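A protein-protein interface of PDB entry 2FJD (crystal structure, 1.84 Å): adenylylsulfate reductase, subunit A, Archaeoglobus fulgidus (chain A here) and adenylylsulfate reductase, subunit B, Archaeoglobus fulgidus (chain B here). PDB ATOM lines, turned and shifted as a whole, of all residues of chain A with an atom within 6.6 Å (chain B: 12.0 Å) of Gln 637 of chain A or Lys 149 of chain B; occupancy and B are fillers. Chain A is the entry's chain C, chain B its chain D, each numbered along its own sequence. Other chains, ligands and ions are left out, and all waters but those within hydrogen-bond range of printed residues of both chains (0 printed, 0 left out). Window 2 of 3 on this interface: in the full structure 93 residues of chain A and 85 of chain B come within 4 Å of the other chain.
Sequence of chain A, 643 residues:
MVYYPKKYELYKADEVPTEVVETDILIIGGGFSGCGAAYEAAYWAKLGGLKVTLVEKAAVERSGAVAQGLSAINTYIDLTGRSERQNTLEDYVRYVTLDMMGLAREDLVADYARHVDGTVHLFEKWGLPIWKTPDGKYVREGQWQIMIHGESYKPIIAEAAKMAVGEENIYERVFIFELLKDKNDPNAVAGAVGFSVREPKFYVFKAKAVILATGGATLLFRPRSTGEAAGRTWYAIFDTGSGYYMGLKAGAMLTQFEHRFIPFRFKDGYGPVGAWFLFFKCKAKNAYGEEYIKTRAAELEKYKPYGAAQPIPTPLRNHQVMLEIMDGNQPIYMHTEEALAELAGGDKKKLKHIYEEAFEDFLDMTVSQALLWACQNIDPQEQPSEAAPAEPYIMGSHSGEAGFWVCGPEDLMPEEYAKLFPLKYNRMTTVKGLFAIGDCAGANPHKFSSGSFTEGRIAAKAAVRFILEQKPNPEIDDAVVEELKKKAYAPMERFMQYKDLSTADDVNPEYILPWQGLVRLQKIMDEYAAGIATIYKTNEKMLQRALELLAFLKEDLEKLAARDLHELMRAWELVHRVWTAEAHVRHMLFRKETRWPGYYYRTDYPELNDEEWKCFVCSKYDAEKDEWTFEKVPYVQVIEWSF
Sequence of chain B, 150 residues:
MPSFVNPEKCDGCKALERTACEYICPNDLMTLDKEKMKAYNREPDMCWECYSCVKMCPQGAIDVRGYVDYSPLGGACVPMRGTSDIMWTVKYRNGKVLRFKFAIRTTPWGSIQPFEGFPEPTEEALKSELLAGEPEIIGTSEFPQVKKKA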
ATOM      1  N   GLU A 106      23.172 -30.270  -6.865  1.00  0.00           N
ATOM      2  CA  GLU A 106      22.130 -30.421  -7.869  1.00  0.00           C
ATOM      3  C   GLU A 106      22.429 -29.796  -9.219  1.00  0.00           C
ATOM      4  O   GLU A 106      21.894 -30.239 -10.236  1.00  0.00           O
ATOM      5  CB  GLU A 106      20.799 -29.908  -7.316  1.00  0.00           C
ATOM      6  CG  GLU A 106      20.414 -30.612  -6.026  1.00  0.00           C
ATOM      7  CD  GLU A 106      19.023 -30.261  -5.548  1.00  0.00           C
ATOM      8  OE1 GLU A 106      18.477 -29.234  -6.007  1.00  0.00           O
ATOM      9  OE2 GLU A 106      18.484 -31.012  -4.703  1.00  0.00           O
ATOM     10  N   TYR A 417      27.775 -21.740  -4.834  1.00  0.00           N
ATOM     11  CA  TYR A 417      28.732 -22.794  -5.174  1.00  0.00           C
ATOM     12  C   TYR A 417      29.907 -22.361  -6.054  1.00  0.00           C
ATOM     13  O   TYR A 417      30.787 -23.165  -6.344  1.00  0.00           O
ATOM     14  CB  TYR A 417      28.002 -23.936  -5.889  1.00  0.00           C
ATOM     15  CG  TYR A 417      26.966 -24.682  -5.068  1.00  0.00           C
ATOM     16  CD1 TYR A 417      26.000 -25.469  -5.696  1.00  0.00           C
ATOM     17  CD2 TYR A 417      26.965 -24.630  -3.671  1.00  0.00           C
ATOM     18  CE1 TYR A 417      25.060 -26.187  -4.963  1.00  0.00           C
ATOM     19  CE2 TYR A 417      26.026 -25.345  -2.923  1.00  0.00           C
ATOM     20  CZ  TYR A 417      25.076 -26.122  -3.581  1.00  0.00           C
ATOM     21  OH  TYR A 417      24.141 -26.835  -2.870  1.00  0.00           O
ATOM     22  N   TYR A 635      24.331 -26.434   1.682  1.00  0.00           N
ATOM     23  CA  TYR A 635      23.595 -26.966   0.552  1.00  0.00           C
ATOM     24  C   TYR A 635      22.452 -26.001   0.255  1.00  0.00           C
ATOM     25  O   TYR A 635      21.865 -25.419   1.170  1.00  0.00           O
ATOM     26  CB  TYR A 635      23.010 -28.343   0.907  1.00  0.00           C
ATOM     27  CG  TYR A 635      21.809 -28.751   0.067  1.00  0.00           C
ATOM     28  CD1 TYR A 635      21.970 -29.437  -1.139  1.00  0.00           C
ATOM     29  CD2 TYR A 635      20.514 -28.418   0.466  1.00  0.00           C
ATOM     30  CE1 TYR A 635      20.862 -29.784  -1.927  1.00  0.00           C
ATOM     31  CE2 TYR A 635      19.407 -28.754  -0.309  1.00  0.00           C
ATOM     32  CZ  TYR A 635      19.585 -29.435  -1.503  1.00  0.00           C
ATOM     33  OH  TYR A 635      18.484 -29.753  -2.261  1.00  0.00           O
ATOM     34  N   VAL A 636      22.163 -25.809  -1.024  1.00  0.00           N
ATOM     35  CA  VAL A 636      21.041 -24.977  -1.435  1.00  0.00           C
ATOM     36  C   VAL A 636      20.354 -25.789  -2.519  1.00  0.00           C
ATOM     37  O   VAL A 636      21.021 -26.415  -3.346  1.00  0.00           O
ATOM     38  CB  VAL A 636      21.472 -23.602  -2.016  1.00  0.00           C
ATOM     39  CG1 VAL A 636      22.000 -22.708  -0.903  1.00  0.00           C
ATOM     40  CG2 VAL A 636      22.514 -23.788  -3.100  1.00  0.00           C
ATOM     41  N   GLN A 637      19.027 -25.817  -2.496  1.00  0.00           N
ATOM     42  CA  GLN A 637      18.290 -26.562  -3.504  1.00  0.00           C
ATOM     43  C   GLN A 637      18.322 -25.745  -4.788  1.00  0.00           C
ATOM     44  O   GLN A 637      17.901 -24.590  -4.805  1.00  0.00           O
ATOM     45  CB  GLN A 637      16.845 -26.787  -3.060  1.00  0.00           C
ATOM     46  CG  GLN A 637      16.113 -27.810  -3.917  1.00  0.00           C
ATOM     47  CD  GLN A 637      14.705 -28.083  -3.429  1.00  0.00           C
ATOM     48  OE1 GLN A 637      14.445 -28.104  -2.226  1.00  0.00           O
ATOM     49  NE2 GLN A 637      13.789 -28.310  -4.365  1.00  0.00           N
ATOM     50  N   VAL A 638      18.831 -26.347  -5.857  1.00  0.00           N
ATOM     51  CA  VAL A 638      18.944 -25.671  -7.141  1.00  0.00           C
ATOM     52  C   VAL A 638      17.783 -25.987  -8.078  1.00  0.00           C
ATOM     53  O   VAL A 638      17.269 -25.106  -8.768  1.00  0.00           O
ATOM     54  CB  VAL A 638      20.271 -26.062  -7.837  1.00  0.00           C
ATOM     55  CG1 VAL A 638      20.373 -25.385  -9.194  1.00  0.00           C
ATOM     56  CG2 VAL A 638      21.450 -25.666  -6.960  1.00  0.00           C
ATOM     57  N   ILE A 639      17.368 -27.249  -8.092  1.00  0.00           N
ATOM     58  CA  ILE A 639      16.286 -27.682  -8.963  1.00  0.00           C
ATOM     59  C   ILE A 639      14.948 -27.724  -8.236  1.00  0.00           C
ATOM     60  O   ILE A 639      14.881 -28.024  -7.042  1.00  0.00           O
ATOM     61  CB  ILE A 639      16.595 -29.073  -9.552  1.00  0.00           C
ATOM     62  CG1 ILE A 639      17.886 -29.003 -10.373  1.00  0.00           C
ATOM     63  CG2 ILE A 639      15.432 -29.562 -10.410  1.00  0.00           C
ATOM     64  CD1 ILE A 639      17.857 -27.980 -11.504  1.00  0.00           C
ATOM     65  N   GLU A 640      13.884 -27.412  -8.967  1.00  0.00           N
ATOM     66  CA  GLU A 640      12.549 -27.410  -8.398  1.00  0.00           C
ATOM     67  C   GLU A 640      12.004 -28.814  -8.167  1.00  0.00           C
ATOM     68  O   GLU A 640      11.863 -29.600  -9.101  1.00  0.00           O
ATOM     69  CB  GLU A 640      11.585 -26.644  -9.307  1.00  0.00           C
ATOM     70  CG  GLU A 640      10.139 -26.702  -8.840  1.00  0.00           C
ATOM     71  CD  GLU A 640       9.198 -25.937  -9.745  1.00  0.00           C
ATOM     72  OE1 GLU A 640       9.347 -24.702  -9.855  1.00  0.00           O
ATOM     73  OE2 GLU A 640       8.310 -26.574 -10.351  1.00  0.00           O
ATOM     74  N   TRP A 641      11.709 -29.114  -6.907  1.00  0.00           N
ATOM     75  CA  TRP A 641      11.138 -30.392  -6.501  1.00  0.00           C
ATOM     76  C   TRP A 641      10.759 -30.302  -5.030  1.00  0.00           C
ATOM     77  O   TRP A 641      11.301 -29.482  -4.288  1.00  0.00           O
ATOM     78  CB  TRP A 641      12.117 -31.561  -6.710  1.00  0.00           C
ATOM     79  CG  TRP A 641      13.394 -31.505  -5.900  1.00  0.00           C
ATOM     80  CD1 TRP A 641      14.609 -31.038  -6.317  1.00  0.00           C
ATOM     81  CD2 TRP A 641      13.584 -31.961  -4.554  1.00  0.00           C
ATOM     82  NE1 TRP A 641      15.542 -31.180  -5.319  1.00  0.00           N
ATOM     83  CE2 TRP A 641      14.940 -31.743  -4.225  1.00  0.00           C
ATOM     84  CE3 TRP A 641      12.738 -32.534  -3.594  1.00  0.00           C
ATOM     85  CZ2 TRP A 641      15.473 -32.077  -2.974  1.00  0.00           C
ATOM     86  CZ3 TRP A 641      13.269 -32.868  -2.346  1.00  0.00           C
ATOM     87  CH2 TRP A 641      14.625 -32.638  -2.050  1.00  0.00           C
ATOM     88  N   SER A 642       9.809 -31.137  -4.627  1.00  0.00           N
ATOM     89  CA  SER A 642       9.358 -31.185  -3.247  1.00  0.00           C
ATOM     90  C   SER A 642       9.211 -32.639  -2.864  1.00  0.00           C
ATOM     91  O   SER A 642       9.009 -33.509  -3.717  1.00  0.00           O
ATOM     92  CB  SER A 642       8.021 -30.458  -3.082  1.00  0.00           C
ATOM     93  OG  SER A 642       7.005 -31.072  -3.852  1.00  0.00           O
ATOM     94  N   GLN B 145      15.170 -29.219 -20.840  1.00  0.00           N
ATOM     95  CA  GLN B 145      15.109 -28.146 -19.854  1.00  0.00           C
ATOM     96  C   GLN B 145      14.822 -28.746 -18.482  1.00  0.00           C
ATOM     97  O   GLN B 145      14.147 -29.772 -18.376  1.00  0.00           O
ATOM     98  CB  GLN B 145      13.997 -27.153 -20.213  1.00  0.00           C
ATOM     99  CG  GLN B 145      14.219 -26.406 -21.518  1.00  0.00           C
ATOM    100  CD  GLN B 145      15.410 -25.472 -21.454  1.00  0.00           C
ATOM    101  OE1 GLN B 145      15.441 -24.545 -20.645  1.00  0.00           O
ATOM    102  NE2 GLN B 145      16.400 -25.712 -22.308  1.00  0.00           N
ATOM    103  N   VAL B 146      15.351 -28.116 -17.439  1.00  0.00           N
ATOM    104  CA  VAL B 146      15.121 -28.572 -16.073  1.00  0.00           C
ATOM    105  C   VAL B 146      14.727 -27.338 -15.256  1.00  0.00           C
ATOM    106  O   VAL B 146      15.418 -26.318 -15.290  1.00  0.00           O
ATOM    107  CB  VAL B 146      16.388 -29.239 -15.475  1.00  0.00           C
ATOM    108  CG1 VAL B 146      17.542 -28.250 -15.454  1.00  0.00           C
ATOM    109  CG2 VAL B 146      16.088 -29.764 -14.071  1.00  0.00           C
ATOM    110  N   LYS B 147      13.604 -27.434 -14.545  1.00  0.00           N
ATOM    111  CA  LYS B 147      13.084 -26.335 -13.740  1.00  0.00           C
ATOM    112  C   LYS B 147      13.957 -25.980 -12.544  1.00  0.00           C
ATOM    113  O   LYS B 147      14.174 -26.801 -11.653  1.00  0.00           O
ATOM    114  CB  LYS B 147      11.675 -26.675 -13.246  1.00  0.00           C
ATOM    115  CG  LYS B 147      10.695 -27.055 -14.349  1.00  0.00           C
ATOM    116  CD  LYS B 147       9.319 -27.366 -13.776  1.00  0.00           C
ATOM    117  CE  LYS B 147       8.331 -27.747 -14.869  1.00  0.00           C
ATOM    118  NZ  LYS B 147       8.755 -28.978 -15.596  1.00  0.00           N
ATOM    119  N   LYS B 148      14.456 -24.750 -12.525  1.00  0.00           N
ATOM    120  CA  LYS B 148      15.279 -24.297 -11.413  1.00  0.00           C
ATOM    121  C   LYS B 148      14.336 -23.847 -10.310  1.00  0.00           C
ATOM    122  O   LYS B 148      13.252 -23.325 -10.583  1.00  0.00           O
ATOM    123  CB  LYS B 148      16.186 -23.146 -11.848  1.00  0.00           C
ATOM    124  CG  LYS B 148      17.232 -23.559 -12.872  1.00  0.00           C
ATOM    125  CD  LYS B 148      18.139 -22.400 -13.272  1.00  0.00           C
ATOM    126  CE  LYS B 148      19.024 -21.963 -12.118  1.00  0.00           C
ATOM    127  NZ  LYS B 148      20.001 -20.914 -12.529  1.00  0.00           N
ATOM    128  N   LYS B 149      14.738 -24.055  -9.064  1.00  0.00           N
ATOM    129  CA  LYS B 149      13.887 -23.676  -7.950  1.00  0.00           C
ATOM    130  C   LYS B 149      13.771 -22.163  -7.832  1.00  0.00           C
ATOM    131  O   LYS B 149      14.771 -21.450  -7.862  1.00  0.00           O
ATOM    132  CB  LYS B 149      14.421 -24.243  -6.638  1.00  0.00           C
ATOM    133  CG  LYS B 149      13.359 -24.255  -5.559  1.00  0.00           C
ATOM    134  CD  LYS B 149      13.939 -24.314  -4.166  1.00  0.00           C
ATOM    135  CE  LYS B 149      12.822 -24.186  -3.142  1.00  0.00           C
ATOM    136  NZ  LYS B 149      13.341 -23.812  -1.802  1.00  0.00           N
ATOM    137  N   ALA B 150      12.539 -21.681  -7.709  1.00  0.00           N
ATOM    138  CA  ALA B 150      12.277 -20.254  -7.583  1.00  0.00           C
ATOM    139  C   ALA B 150      12.922 -19.690  -6.320  1.00  0.00           C
ATOM    140  O   ALA B 150      12.189 -19.477  -5.332  1.00  0.00           O
ATOM    141  CB  ALA B 150      10.773 -20.001  -7.565  1.00  0.00           C
ATOM    142  OXT ALA B 150      14.154 -19.487  -6.328  1.00  0.00           O
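The backbone NH (N) of Val 638 of chain A sits at hydrogen-bond distance from the side-chain carboxylate (OE1) of Glu 106 of chain A.
OE1 of Glu 106 of chain A sits at hydrogen-bond distance from N of Ile 639 of chain A (3.1 Å).
NE2 of Gln 637 of chain A is in hydrogen-bond range of O of Ile 639 of chain A, 2.9 Å away.
O of Trp 641 of chain A is in hydrogen-bond range of NE2 of Gln 637 of chain A (2.8 Å).
Among the printed residues, no Asp or Glu carboxylate lies within 4 Å of a Lys or Arg side-chain nitrogen of the other chain.
The backbone NH (N) of Lys 149 of chain B is in hydrogen-bond range of the backbone carbonyl oxygen (O) of Val 638 of chain A.
The backbone NH (N) of Glu 640 of chain A lies within hydrogen-bond range of the backbone carbonyl oxygen (O) of Lys 147 of chain B, 2.8 Å away.
The backbone NH of Glu 640 of chain A lies close to the backbone NH of Lys 149 of chain B.
Gln 637 of chain A touches Lys 149 of chain B.
Val 638 of chain A touches Lys 148 of chain B.
Val 146 of chain B touches Ile 639 of chain A (CG2 to CD1, 3.6 Å).
Ile 639 of chain A touches Lys 147 of chain B (CG2 to O, 3.3 Å).
C of Ile 639 of chain A touches N of Lys 149 of chain B, 3.8 Å away.
C of Lys 148 of chain B touches N of Glu 640 of chain A (3.8 Å).
Gln 637 of chain A touches just one residue of chain B: Lys 149.
No residue of chain B comes within 4 Å of Glu 106 of chain A.
Of chain B, only Lys 148 (3.4 Å) and Lys 149 (2.8 Å) come within 4 Å of Val 638 of chain A.
Ile 639 of chain A touches just these residues of chain B: Val 146 (3.6 Å), Lys 147 (3.3 Å) and Lys 149 (3.8 Å).
No residue of chain B comes within 4 Å of Trp 641 of chain A.
Of the printed residues of chain A, Lys 148 of chain B touches Val 638 (3.4 Å) and Glu 640 (3.8 Å).
Printed residues of chain A within 4 Å of Lys 147 of chain B: Ile 639 and Glu 640.
Printed residues of chain A within 4 Å of Val 146 of chain B: Ile 639 (3.6 Å).
The nearest residue of chain A that does not touch Lys 149 of chain B is Trp 641 of chain A (5.3 Å).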
